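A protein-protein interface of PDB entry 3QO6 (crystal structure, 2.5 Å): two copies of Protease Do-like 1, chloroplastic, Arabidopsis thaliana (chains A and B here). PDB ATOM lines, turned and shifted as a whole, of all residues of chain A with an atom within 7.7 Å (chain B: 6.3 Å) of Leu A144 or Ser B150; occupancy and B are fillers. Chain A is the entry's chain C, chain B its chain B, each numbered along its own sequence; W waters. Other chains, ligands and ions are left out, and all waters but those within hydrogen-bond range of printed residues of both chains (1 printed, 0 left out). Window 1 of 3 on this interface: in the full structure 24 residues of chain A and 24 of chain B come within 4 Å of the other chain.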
ATOM      1  N   THR A  19      18.045  -7.477  33.573  1.00  0.00           N
ATOM      2  CA  THR A  19      18.955  -7.067  32.531  1.00  0.00           C
ATOM      3  C   THR A  19      18.567  -7.750  31.235  1.00  0.00           C
ATOM      4  O   THR A  19      18.659  -7.142  30.166  1.00  0.00           O
ATOM      5  CB  THR A  19      20.450  -7.255  32.930  1.00  0.00           C
ATOM      6  OG1 THR A  19      21.111  -8.035  31.950  1.00  0.00           O
ATOM      7  CG2 THR A  19      20.580  -7.849  34.267  1.00  0.00           C
ATOM      8  N   VAL A  20      18.064  -8.976  31.320  1.00  0.00           N
ATOM      9  CA  VAL A  20      17.609  -9.669  30.110  1.00  0.00           C
ATOM     10  C   VAL A  20      16.411  -8.930  29.473  1.00  0.00           C
ATOM     11  O   VAL A  20      16.347  -8.814  28.252  1.00  0.00           O
ATOM     12  CB  VAL A  20      17.241 -11.175  30.386  1.00  0.00           C
ATOM     13  CG1 VAL A  20      16.286 -11.714  29.312  1.00  0.00           C
ATOM     14  CG2 VAL A  20      18.506 -12.024  30.361  1.00  0.00           C
ATOM     15  N   LEU A  22      15.580  -5.612  29.833  1.00  0.00           N
ATOM     16  CA  LEU A  22      16.089  -4.341  29.344  1.00  0.00           C
ATOM     17  C   LEU A  22      16.704  -4.526  27.969  1.00  0.00           C
ATOM     18  O   LEU A  22      16.489  -3.710  27.060  1.00  0.00           O
ATOM     19  CB  LEU A  22      17.102  -3.776  30.327  1.00  0.00           C
ATOM     20  CG  LEU A  22      17.849  -2.487  29.997  1.00  0.00           C
ATOM     21  CD1 LEU A  22      18.289  -1.868  31.316  1.00  0.00           C
ATOM     22  CD2 LEU A  22      19.072  -2.751  29.108  1.00  0.00           C
ATOM     23  N   PHE A  23      17.439  -5.621  27.790  1.00  0.00           N
ATOM     24  CA  PHE A  23      18.067  -5.853  26.495  1.00  0.00           C
ATOM     25  C   PHE A  23      17.102  -6.250  25.379  1.00  0.00           C
ATOM     26  O   PHE A  23      17.235  -5.768  24.265  1.00  0.00           O
ATOM     27  CB  PHE A  23      19.173  -6.902  26.599  1.00  0.00           C
ATOM     28  CG  PHE A  23      19.899  -7.105  25.319  1.00  0.00           C
ATOM     29  CD1 PHE A  23      20.876  -6.197  24.918  1.00  0.00           C
ATOM     30  CD2 PHE A  23      19.523  -8.130  24.452  1.00  0.00           C
ATOM     31  CE1 PHE A  23      21.454  -6.295  23.681  1.00  0.00           C
ATOM     32  CE2 PHE A  23      20.096  -8.245  23.205  1.00  0.00           C
ATOM     33  CZ  PHE A  23      21.063  -7.318  22.814  1.00  0.00           C
ATOM     34  N   GLN A  24      16.153  -7.145  25.660  1.00  0.00           N
ATOM     35  CA  GLN A  24      15.185  -7.550  24.648  1.00  0.00           C
ATOM     36  C   GLN A  24      14.462  -6.322  24.182  1.00  0.00           C
ATOM     37  O   GLN A  24      14.316  -6.089  22.986  1.00  0.00           O
ATOM     38  CB  GLN A  24      14.168  -8.528  25.219  1.00  0.00           C
ATOM     39  CG  GLN A  24      14.735  -9.900  25.338  1.00  0.00           C
ATOM     40  CD  GLN A  24      13.872 -10.855  26.132  1.00  0.00           C
ATOM     41  OE1 GLN A  24      13.250 -10.485  27.151  1.00  0.00           O
ATOM     42  NE2 GLN A  24      13.851 -12.113  25.691  1.00  0.00           N
ATOM     43  N   THR A  27      17.473  -3.489  22.399  1.00  0.00           N
ATOM     44  CA  THR A  27      18.350  -3.766  21.281  1.00  0.00           C
ATOM     45  C   THR A  27      17.726  -3.384  19.917  1.00  0.00           C
ATOM     46  O   THR A  27      18.415  -2.854  19.034  1.00  0.00           O
ATOM     47  CB  THR A  27      18.848  -5.262  21.286  1.00  0.00           C
ATOM     48  OG1 THR A  27      19.794  -5.461  20.230  1.00  0.00           O
ATOM     49  CG2 THR A  27      17.729  -6.218  21.090  1.00  0.00           C
ATOM     50  N   VAL A 131      24.550   0.583  34.997  1.00  0.00           N
ATOM     51  CA  VAL A 131      24.384   1.026  33.605  1.00  0.00           C
ATOM     52  C   VAL A 131      24.498  -0.113  32.587  1.00  0.00           C
ATOM     53  O   VAL A 131      25.064  -1.163  32.879  1.00  0.00           O
ATOM     54  CB  VAL A 131      25.384   2.163  33.193  1.00  0.00           C
ATOM     55  CG1 VAL A 131      25.288   3.308  34.164  1.00  0.00           C
ATOM     56  CG2 VAL A 131      26.782   1.635  33.093  1.00  0.00           C
ATOM     57  N   PHE A 132      23.974   0.129  31.385  1.00  0.00           N
ATOM     58  CA  PHE A 132      23.918  -0.859  30.329  1.00  0.00           C
ATOM     59  C   PHE A 132      24.324  -0.258  29.004  1.00  0.00           C
ATOM     60  O   PHE A 132      23.685   0.679  28.513  1.00  0.00           O
ATOM     61  CB  PHE A 132      22.485  -1.386  30.221  1.00  0.00           C
ATOM     62  CG  PHE A 132      21.955  -1.925  31.509  1.00  0.00           C
ATOM     63  CD1 PHE A 132      22.043  -3.298  31.791  1.00  0.00           C
ATOM     64  CD2 PHE A 132      21.507  -1.048  32.512  1.00  0.00           C
ATOM     65  CE1 PHE A 132      21.713  -3.799  33.055  1.00  0.00           C
ATOM     66  CE2 PHE A 132      21.171  -1.526  33.800  1.00  0.00           C
ATOM     67  CZ  PHE A 132      21.278  -2.902  34.071  1.00  0.00           C
ATOM     68  N   ALA A 133      25.365  -0.809  28.395  1.00  0.00           N
ATOM     69  CA  ALA A 133      25.816  -0.269  27.116  1.00  0.00           C
ATOM     70  C   ALA A 133      25.563  -1.214  25.974  1.00  0.00           C
ATOM     71  O   ALA A 133      25.928  -2.388  26.050  1.00  0.00           O
ATOM     72  CB  ALA A 133      27.323   0.085  27.187  1.00  0.00           C
ATOM     73  N   ILE A 134      24.925  -0.720  24.920  1.00  0.00           N
ATOM     74  CA  ILE A 134      24.711  -1.544  23.732  1.00  0.00           C
ATOM     75  C   ILE A 134      25.355  -0.886  22.534  1.00  0.00           C
ATOM     76  O   ILE A 134      25.127   0.310  22.288  1.00  0.00           O
ATOM     77  CB  ILE A 134      23.250  -1.714  23.382  1.00  0.00           C
ATOM     78  CG1 ILE A 134      22.487  -2.235  24.612  1.00  0.00           C
ATOM     79  CG2 ILE A 134      23.146  -2.618  22.133  1.00  0.00           C
ATOM     80  CD1 ILE A 134      20.982  -2.513  24.371  1.00  0.00           C
ATOM     81  N   GLY A 135      26.139  -1.668  21.785  1.00  0.00           N
ATOM     82  CA  GLY A 135      26.809  -1.177  20.583  1.00  0.00           C
ATOM     83  C   GLY A 135      27.414  -2.290  19.726  1.00  0.00           C
ATOM     84  O   GLY A 135      27.022  -3.462  19.815  1.00  0.00           O
ATOM     85  N   ASN A 136      28.402  -1.940  18.905  1.00  0.00           N
ATOM     86  CA  ASN A 136      29.038  -2.926  18.036  1.00  0.00           C
ATOM     87  C   ASN A 136      30.554  -2.952  18.133  1.00  0.00           C
ATOM     88  O   ASN A 136      31.264  -2.806  17.147  1.00  0.00           O
ATOM     89  CB  ASN A 136      28.603  -2.683  16.591  1.00  0.00           C
ATOM     90  CG  ASN A 136      27.118  -2.355  16.495  1.00  0.00           C
ATOM     91  OD1 ASN A 136      26.265  -3.204  16.803  1.00  0.00           O
ATOM     92  ND2 ASN A 136      26.798  -1.108  16.105  1.00  0.00           N
ATOM     93  N   PRO A 137      31.076  -3.157  19.337  1.00  0.00           N
ATOM     94  CA  PRO A 137      32.540  -3.202  19.484  1.00  0.00           C
ATOM     95  C   PRO A 137      33.169  -4.262  18.545  1.00  0.00           C
ATOM     96  O   PRO A 137      32.728  -5.425  18.496  1.00  0.00           O
ATOM     97  CB  PRO A 137      32.723  -3.571  20.953  1.00  0.00           C
ATOM     98  CG  PRO A 137      31.495  -4.419  21.241  1.00  0.00           C
ATOM     99  CD  PRO A 137      30.388  -3.647  20.549  1.00  0.00           C
ATOM    100  N   LEU A 140      31.056  -6.632  16.587  1.00  0.00           N
ATOM    101  CA  LEU A 140      30.186  -7.608  17.222  1.00  0.00           C
ATOM    102  C   LEU A 140      28.779  -7.033  17.452  1.00  0.00           C
ATOM    103  O   LEU A 140      28.530  -6.351  18.455  1.00  0.00           O
ATOM    104  CB  LEU A 140      30.812  -8.059  18.539  1.00  0.00           C
ATOM    105  CG  LEU A 140      32.054  -8.926  18.365  1.00  0.00           C
ATOM    106  CD1 LEU A 140      32.908  -8.823  19.613  1.00  0.00           C
ATOM    107  CD2 LEU A 140      31.657 -10.369  18.089  1.00  0.00           C
ATOM    108  N   ASP A 141      27.872  -7.333  16.524  1.00  0.00           N
ATOM    109  CA  ASP A 141      26.481  -6.865  16.516  1.00  0.00           C
ATOM    110  C   ASP A 141      25.657  -6.772  17.821  1.00  0.00           C
ATOM    111  O   ASP A 141      25.314  -7.780  18.433  1.00  0.00           O
ATOM    112  CB  ASP A 141      25.705  -7.713  15.523  1.00  0.00           C
ATOM    113  CG  ASP A 141      24.708  -6.909  14.741  1.00  0.00           C
ATOM    114  OD1 ASP A 141      25.143  -5.912  14.123  1.00  0.00           O
ATOM    115  OD2 ASP A 141      23.506  -7.264  14.732  1.00  0.00           O
ATOM    116  N   HIS A 142      25.292  -5.550  18.207  1.00  0.00           N
ATOM    117  CA  HIS A 142      24.501  -5.297  19.412  1.00  0.00           C
ATOM    118  C   HIS A 142      24.988  -6.003  20.683  1.00  0.00           C
ATOM    119  O   HIS A 142      24.230  -6.693  21.374  1.00  0.00           O
ATOM    120  CB  HIS A 142      23.022  -5.611  19.170  1.00  0.00           C
ATOM    121  CG  HIS A 142      22.385  -4.766  18.102  1.00  0.00           C
ATOM    122  ND1 HIS A 142      21.046  -4.430  18.121  1.00  0.00           N
ATOM    123  CD2 HIS A 142      22.895  -4.219  16.968  1.00  0.00           C
ATOM    124  CE1 HIS A 142      20.758  -3.714  17.046  1.00  0.00           C
ATOM    125  NE2 HIS A 142      21.860  -3.573  16.329  1.00  0.00           N
ATOM    126  N   THR A 143      26.268  -5.796  20.976  1.00  0.00           N
ATOM    127  CA  THR A 143      26.920  -6.341  22.155  1.00  0.00           C
ATOM    128  C   THR A 143      26.417  -5.602  23.383  1.00  0.00           C
ATOM    129  O   THR A 143      26.337  -4.358  23.396  1.00  0.00           O
ATOM    130  CB  THR A 143      28.460  -6.111  22.107  1.00  0.00           C
ATOM    131  OG1 THR A 143      29.057  -7.004  21.158  1.00  0.00           O
ATOM    132  CG2 THR A 143      29.074  -6.288  23.478  1.00  0.00           C
ATOM    133  N   LEU A 144      26.082  -6.362  24.414  1.00  0.00           N
ATOM    134  CA  LEU A 144      25.651  -5.766  25.660  1.00  0.00           C
ATOM    135  C   LEU A 144      26.767  -5.891  26.680  1.00  0.00           C
ATOM    136  O   LEU A 144      27.270  -7.001  26.883  1.00  0.00           O
ATOM    137  CB  LEU A 144      24.439  -6.485  26.235  1.00  0.00           C
ATOM    138  CG  LEU A 144      24.150  -6.143  27.707  1.00  0.00           C
ATOM    139  CD1 LEU A 144      23.620  -4.745  27.818  1.00  0.00           C
ATOM    140  CD2 LEU A 144      23.134  -7.110  28.294  1.00  0.00           C
ATOM    141  N   THR A 145      27.163  -4.771  27.293  1.00  0.00           N
ATOM    142  CA  THR A 145      28.146  -4.814  28.361  1.00  0.00           C
ATOM    143  C   THR A 145      27.548  -4.047  29.501  1.00  0.00           C
ATOM    144  O   THR A 145      26.892  -3.026  29.318  1.00  0.00           O
ATOM    145  CB  THR A 145      29.491  -4.222  27.984  1.00  0.00           C
ATOM    146  OG1 THR A 145      29.306  -2.911  27.439  1.00  0.00           O
ATOM    147  CG2 THR A 145      30.188  -5.131  26.979  1.00  0.00           C
ATOM    148  N   THR A 146      27.797  -4.564  30.690  1.00  0.00           N
ATOM    149  CA  THR A 146      27.271  -4.061  31.945  1.00  0.00           C
ATOM    150  C   THR A 146      28.307  -3.426  32.855  1.00  0.00           C
ATOM    151  O   THR A 146      29.470  -3.813  32.853  1.00  0.00           O
ATOM    152  CB  THR A 146      26.606  -5.257  32.671  1.00  0.00           C
ATOM    153  OG1 THR A 146      25.238  -5.298  32.300  1.00  0.00           O
ATOM    154  CG2 THR A 146      26.765  -5.215  34.161  1.00  0.00           C
ATOM    155  N   GLY A 147      27.864  -2.474  33.663  1.00  0.00           N
ATOM    156  CA  GLY A 147      28.746  -1.804  34.595  1.00  0.00           C
ATOM    157  C   GLY A 147      27.976  -0.882  35.524  1.00  0.00           C
ATOM    158  O   GLY A 147      26.770  -0.977  35.704  1.00  0.00           O
ATOM    159  N   ALA A 173      31.570  -0.100  32.418  1.00  0.00           N
ATOM    160  CA  ALA A 173      31.006  -1.113  31.547  1.00  0.00           C
ATOM    161  C   ALA A 173      31.996  -1.107  30.373  1.00  0.00           C
ATOM    162  O   ALA A 173      32.457  -0.029  29.963  1.00  0.00           O
ATOM    163  CB  ALA A 173      29.641  -0.716  31.088  1.00  0.00           C
ATOM    164  N   ALA A 174      32.351  -2.287  29.853  1.00  0.00           N
ATOM    165  CA  ALA A 174      33.320  -2.377  28.748  1.00  0.00           C
ATOM    166  C   ALA A 174      32.885  -1.589  27.517  1.00  0.00           C
ATOM    167  O   ALA A 174      31.795  -1.802  26.967  1.00  0.00           O
ATOM    168  CB  ALA A 174      33.583  -3.861  28.371  1.00  0.00           C
ATOM    169  N   ASN A 179      31.865   0.855  19.688  1.00  0.00           N
ATOM    170  CA  ASN A 179      30.810   1.252  20.622  1.00  0.00           C
ATOM    171  C   ASN A 179      30.369   2.721  20.400  1.00  0.00           C
ATOM    172  O   ASN A 179      29.212   3.062  20.644  1.00  0.00           O
ATOM    173  CB  ASN A 179      31.312   1.106  22.070  1.00  0.00           C
ATOM    174  CG  ASN A 179      30.891  -0.218  22.735  1.00  0.00           C
ATOM    175  OD1 ASN A 179      29.682  -0.498  22.937  1.00  0.00           O
ATOM    176  ND2 ASN A 179      31.890  -1.019  23.111  1.00  0.00           N
ATOM    177  N   PRO A 183      23.866   3.605  22.626  1.00  0.00           N
ATOM    178  CA  PRO A 183      23.278   4.023  23.889  1.00  0.00           C
ATOM    179  C   PRO A 183      23.846   3.481  25.171  1.00  0.00           C
ATOM    180  O   PRO A 183      24.375   2.365  25.207  1.00  0.00           O
ATOM    181  CB  PRO A 183      21.827   3.593  23.729  1.00  0.00           C
ATOM    182  CG  PRO A 183      21.993   2.286  23.028  1.00  0.00           C
ATOM    183  CD  PRO A 183      23.011   2.623  21.942  1.00  0.00           C
ATOM    184  N   LEU A 185      22.211   2.950  28.855  1.00  0.00           N
ATOM    185  CA  LEU A 185      20.926   2.958  29.530  1.00  0.00           C
ATOM    186  C   LEU A 185      21.050   2.816  31.054  1.00  0.00           C
ATOM    187  O   LEU A 185      22.039   2.245  31.553  1.00  0.00           O
ATOM    188  CB  LEU A 185      20.074   1.822  28.986  1.00  0.00           C
ATOM    189  CG  LEU A 185      19.918   1.795  27.469  1.00  0.00           C
ATOM    190  CD1 LEU A 185      19.251   0.509  27.091  1.00  0.00           C
ATOM    191  CD2 LEU A 185      19.102   2.938  26.970  1.00  0.00           C
ATOM    192  N   VAL B 127      21.015 -13.011  26.033  1.00  0.00           N
ATOM    193  CA  VAL B 127      21.936 -11.906  26.333  1.00  0.00           C
ATOM    194  C   VAL B 127      21.474 -11.217  27.612  1.00  0.00           C
ATOM    195  O   VAL B 127      20.279 -10.936  27.782  1.00  0.00           O
ATOM    196  CB  VAL B 127      21.951 -10.865  25.218  1.00  0.00           C
ATOM    197  CG1 VAL B 127      22.660  -9.587  25.688  1.00  0.00           C
ATOM    198  CG2 VAL B 127      22.652 -11.448  24.022  1.00  0.00           C
ATOM    199  N   GLY B 128      22.407 -10.957  28.520  1.00  0.00           N
ATOM    200  CA  GLY B 128      22.038 -10.301  29.761  1.00  0.00           C
ATOM    201  C   GLY B 128      22.078 -11.222  30.971  1.00  0.00           C
ATOM    202  O   GLY B 128      22.233 -10.733  32.096  1.00  0.00           O
ATOM    203  N   GLN B 129      21.947 -12.541  30.805  1.00  0.00           N
ATOM    204  CA  GLN B 129      21.976 -13.368  32.026  1.00  0.00           C
ATOM    205  C   GLN B 129      23.395 -13.431  32.564  1.00  0.00           C
ATOM    206  O   GLN B 129      24.342 -13.273  31.799  1.00  0.00           O
ATOM    207  CB  GLN B 129      21.391 -14.764  31.784  1.00  0.00           C
ATOM    208  CG  GLN B 129      22.098 -15.607  30.791  1.00  0.00           C
ATOM    209  CD  GLN B 129      21.358 -16.932  30.556  1.00  0.00           C
ATOM    210  OE1 GLN B 129      20.687 -17.102  29.524  1.00  0.00           O
ATOM    211  NE2 GLN B 129      21.472 -17.871  31.514  1.00  0.00           N
ATOM    212  N   VAL B 148      28.465 -10.877  32.115  1.00  0.00           N
ATOM    213  CA  VAL B 148      27.168 -11.153  31.543  1.00  0.00           C
ATOM    214  C   VAL B 148      27.326 -11.785  30.135  1.00  0.00           C
ATOM    215  O   VAL B 148      28.403 -11.717  29.525  1.00  0.00           O
ATOM    216  CB  VAL B 148      26.436  -9.764  31.502  1.00  0.00           C
ATOM    217  CG1 VAL B 148      26.263  -9.277  30.045  1.00  0.00           C
ATOM    218  CG2 VAL B 148      25.179  -9.800  32.301  1.00  0.00           C
ATOM    219  N   ILE B 149      26.295 -12.444  29.628  1.00  0.00           N
ATOM    220  CA  ILE B 149      26.403 -12.943  28.266  1.00  0.00           C
ATOM    221  C   ILE B 149      26.209 -11.665  27.445  1.00  0.00           C
ATOM    222  O   ILE B 149      25.170 -11.014  27.565  1.00  0.00           O
ATOM    223  CB  ILE B 149      25.258 -13.893  27.890  1.00  0.00           C
ATOM    224  CG1 ILE B 149      25.449 -15.253  28.566  1.00  0.00           C
ATOM    225  CG2 ILE B 149      25.163 -13.982  26.362  1.00  0.00           C
ATOM    226  CD1 ILE B 149      24.586 -16.334  27.971  1.00  0.00           C
ATOM    227  N   SER B 150      27.190 -11.306  26.626  1.00  0.00           N
ATOM    228  CA  SER B 150      27.127 -10.090  25.828  1.00  0.00           C
ATOM    229  C   SER B 150      26.547 -10.327  24.469  1.00  0.00           C
ATOM    230  O   SER B 150      26.048  -9.394  23.814  1.00  0.00           O
ATOM    231  CB  SER B 150      28.520  -9.510  25.631  1.00  0.00           C
ATOM    232  OG  SER B 150      29.048  -9.042  26.847  1.00  0.00           O
ATOM    233  N   GLY B 151      26.657 -11.572  24.030  1.00  0.00           N
ATOM    234  CA  GLY B 151      26.179 -11.938  22.711  1.00  0.00           C
ATOM    235  C   GLY B 151      26.108 -13.440  22.518  1.00  0.00           C
ATOM    236  O   GLY B 151      26.746 -14.241  23.238  1.00  0.00           O
ATOM    237  N   LEU B 152      25.314 -13.820  21.526  1.00  0.00           N
ATOM    238  CA  LEU B 152      25.119 -15.216  21.194  1.00  0.00           C
ATOM    239  C   LEU B 152      25.262 -15.439  19.700  1.00  0.00           C
ATOM    240  O   LEU B 152      25.190 -14.496  18.916  1.00  0.00           O
ATOM    241  CB  LEU B 152      23.736 -15.647  21.666  1.00  0.00           C
ATOM    242  CG  LEU B 152      23.739 -15.615  23.185  1.00  0.00           C
ATOM    243  CD1 LEU B 152      22.336 -15.736  23.760  1.00  0.00           C
ATOM    244  CD2 LEU B 152      24.663 -16.754  23.660  1.00  0.00           C
ATOM    245  N   ARG B 154      27.797 -15.950  17.773  1.00  0.00           N
ATOM    246  CA  ARG B 154      28.875 -15.209  17.123  1.00  0.00           C
ATOM    247  C   ARG B 154      29.757 -16.181  16.362  1.00  0.00           C
ATOM    248  O   ARG B 154      29.818 -17.359  16.717  1.00  0.00           O
ATOM    249  CB  ARG B 154      29.774 -14.513  18.158  1.00  0.00           C
ATOM    250  CG  ARG B 154      29.073 -13.625  19.168  1.00  0.00           C
ATOM    251  CD  ARG B 154      28.302 -12.497  18.496  1.00  0.00           C
ATOM    252  NE  ARG B 154      28.124 -11.368  19.400  1.00  0.00           N
ATOM    253  CZ  ARG B 154      27.358 -10.305  19.153  1.00  0.00           C
ATOM    254  NH1 ARG B 154      26.674 -10.209  18.017  1.00  0.00           N
ATOM    255  NH2 ARG B 154      27.290  -9.329  20.045  1.00  0.00           N
ATOM    256  N   ILE B 169      29.852 -18.034  22.212  1.00  0.00           N
ATOM    257  CA  ILE B 169      29.291 -17.159  23.256  1.00  0.00           C
ATOM    258  C   ILE B 169      30.242 -15.977  23.557  1.00  0.00           C
ATOM    259  O   ILE B 169      31.455 -16.158  23.588  1.00  0.00           O
ATOM    260  CB  ILE B 169      29.092 -17.895  24.583  1.00  0.00           C
ATOM    261  CG1 ILE B 169      28.059 -19.014  24.432  1.00  0.00           C
ATOM    262  CG2 ILE B 169      28.637 -16.900  25.642  1.00  0.00           C
ATOM    263  CD1 ILE B 169      28.013 -19.952  25.631  1.00  0.00           C
ATOM    264  N   GLN B 170      29.682 -14.784  23.779  1.00  0.00           N
ATOM    265  CA  GLN B 170      30.461 -13.578  24.077  1.00  0.00           C
ATOM    266  C   GLN B 170      30.126 -13.094  25.490  1.00  0.00           C
ATOM    267  O   GLN B 170      28.954 -13.007  25.850  1.00  0.00           O
ATOM    268  CB  GLN B 170      30.112 -12.490  23.084  1.00  0.00           C
ATOM    269  CG  GLN B 170      31.038 -11.332  23.122  1.00  0.00           C
ATOM    270  CD  GLN B 170      30.586 -10.243  22.197  1.00  0.00           C
ATOM    271  OE1 GLN B 170      30.137 -10.510  21.092  1.00  0.00           O
ATOM    272  NE2 GLN B 170      30.703  -9.003  22.638  1.00  0.00           N
ATOM    273  N   THR B 171      31.148 -12.788  26.286  1.00  0.00           N
ATOM    274  CA  THR B 171      30.943 -12.361  27.659  1.00  0.00           C
ATOM    275  C   THR B 171      31.922 -11.252  28.036  1.00  0.00           C
ATOM    276  O   THR B 171      33.033 -11.161  27.467  1.00  0.00           O
ATOM    277  CB  THR B 171      31.148 -13.522  28.644  1.00  0.00           C
ATOM    278  OG1 THR B 171      30.856 -13.071  29.966  1.00  0.00           O
ATOM    279  CG2 THR B 171      32.602 -14.000  28.634  1.00  0.00           C
ATOM    280  N   ASP B 172      31.512 -10.412  28.989  1.00  0.00           N
ATOM    281  CA  ASP B 172      32.361  -9.317  29.405  1.00  0.00           C
ATOM    282  C   ASP B 172      33.003  -9.617  30.735  1.00  0.00           C
ATOM    283  O   ASP B 172      33.559  -8.725  31.392  1.00  0.00           O
ATOM    284  CB  ASP B 172      31.605  -7.972  29.409  1.00  0.00           C
ATOM    285  CG  ASP B 172      30.422  -7.936  30.371  1.00  0.00           C
ATOM    286  OD1 ASP B 172      30.031  -9.003  30.905  1.00  0.00           O
ATOM    287  OD2 ASP B 172      29.874  -6.818  30.588  1.00  0.00           O
ATOM    288  N   ALA B 173      32.936 -10.894  31.113  1.00  0.00           N
ATOM    289  CA  ALA B 173      33.592 -11.373  32.322  1.00  0.00           C
ATOM    290  C   ALA B 173      35.064 -11.381  31.934  1.00  0.00           C
ATOM    291  O   ALA B 173      35.411 -11.869  30.856  1.00  0.00           O
ATOM    292  CB  ALA B 173      33.164 -12.791  32.636  1.00  0.00           C
ATOM    293  N   GLY B 207      37.287  -6.942  27.910  1.00  0.00           N
ATOM    294  CA  GLY B 207      35.853  -7.072  28.011  1.00  0.00           C
ATOM    295  C   GLY B 207      35.098  -7.764  26.883  1.00  0.00           C
ATOM    296  O   GLY B 207      33.866  -7.754  26.890  1.00  0.00           O
HETATM  297  O   HOH W   1      31.486  -4.713  31.056  1.00  0.00           O
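O of Gly B128 is in hydrogen-bond range of OG1 of Thr A19 (2.9 Å).
OG of Ser B150 sits at hydrogen-bond distance from O of Leu A144 (2.7 Å).
The guanidinium group (NH1) of Arg B154 lies within hydrogen-bond range of the backbone carbonyl oxygen (O) of Asp A141 (2.8 Å).
The side-chain hydroxyl (OG1) of Thr A143 lies within hydrogen-bond range of the guanidinium group (NH2) of Arg B154, 3.1 Å away.
The side-chain amide nitrogen of Gln B170 lies within hydrogen-bond range of the side-chain hydroxyl of Thr A143 (3.0 Å).
The side-chain carboxylate (OD2) of Asp B172 is in hydrogen-bond range of the backbone NH (N) of Thr A146, at 3.1 Å.
O of Ile B149 is in hydrogen-bond range of N of Gly B128 (2.9 Å).
N of Val B148 lies within hydrogen-bond range of OD1 of Asp B172 (2.7 Å).
O of Gln B170 is in hydrogen-bond range of N of Ser B150 (2.6 Å).
The side-chain amide oxygen (OE1) of Gln B170 sits at hydrogen-bond distance from the guanidinium group (NE) of Arg B154 (2.8 Å).
The backbone NH (N) of Ala A133 lies within hydrogen-bond range of the backbone carbonyl oxygen (O) of Thr A145 (2.8 Å).
O of Gly A135 sits at hydrogen-bond distance from N of Thr A143 (2.7 Å).
Gly B128 touches Val A20 (C to CG2, 3.7 Å).
Val A20 touches Gln B129 (CG2 to N, 3.5 Å).
Val B127 touches Phe A23 (CG1 to CD2, 3.7 Å).
Arg B154 touches Leu A140.
Leu A140 touches Gln B170.
Thr A143 touches Ser B150 (CA to O, 3.6 Å).
Leu A144 touches Val B127.
Leu A144 touches Gly B128.
CA of Thr A145 touches OD2 of Asp B172, at 3.5 Å.
Ala A174 touches Gly B207.
Leu A22 touches none of the printed residues of chain B.
Of the printed residues of chain B, Phe A23 touches Val B127 (3.7 Å).
Leu A144 touches three residues of chain B.
Printed residues of chain B within 4 Å of Thr A146: Asp B172 (3.1 Å).
Gly A147 touches none of the printed residues of chain B.
Of the printed residues of chain A, Ser B150 touches Thr A143 (3.6 Å) and Leu A144 (2.7 Å).
The nearest residue of chain B that does not touch Leu A144 is Val B148 (4.02 Å).
The nearest printed residue of chain A that does not touch Ser B150 is His A142 (4.1 Å).
Hydrophobic or aromatic side chains of chain B that line the printed part of chain A: Val B127.
Hydrophobic or aromatic side chains of chain A that line the printed part of chain B: Val A20, Phe A23, Leu A140, Leu A144 and Ala A174.
Among the printed residues, no Asp or Glu carboxylate lies within 4 Å of a Lys or Arg side-chain nitrogen of the other chain.
1 position is printed for both chains.
Of the 17 pairs that touch across the chains among the printed residues, none has its exchanged pair printed and touching as well.
Water W1 lies within hydrogen-bond range of OD2 of Asp B172, N of Ala A174 and O of Thr A146.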
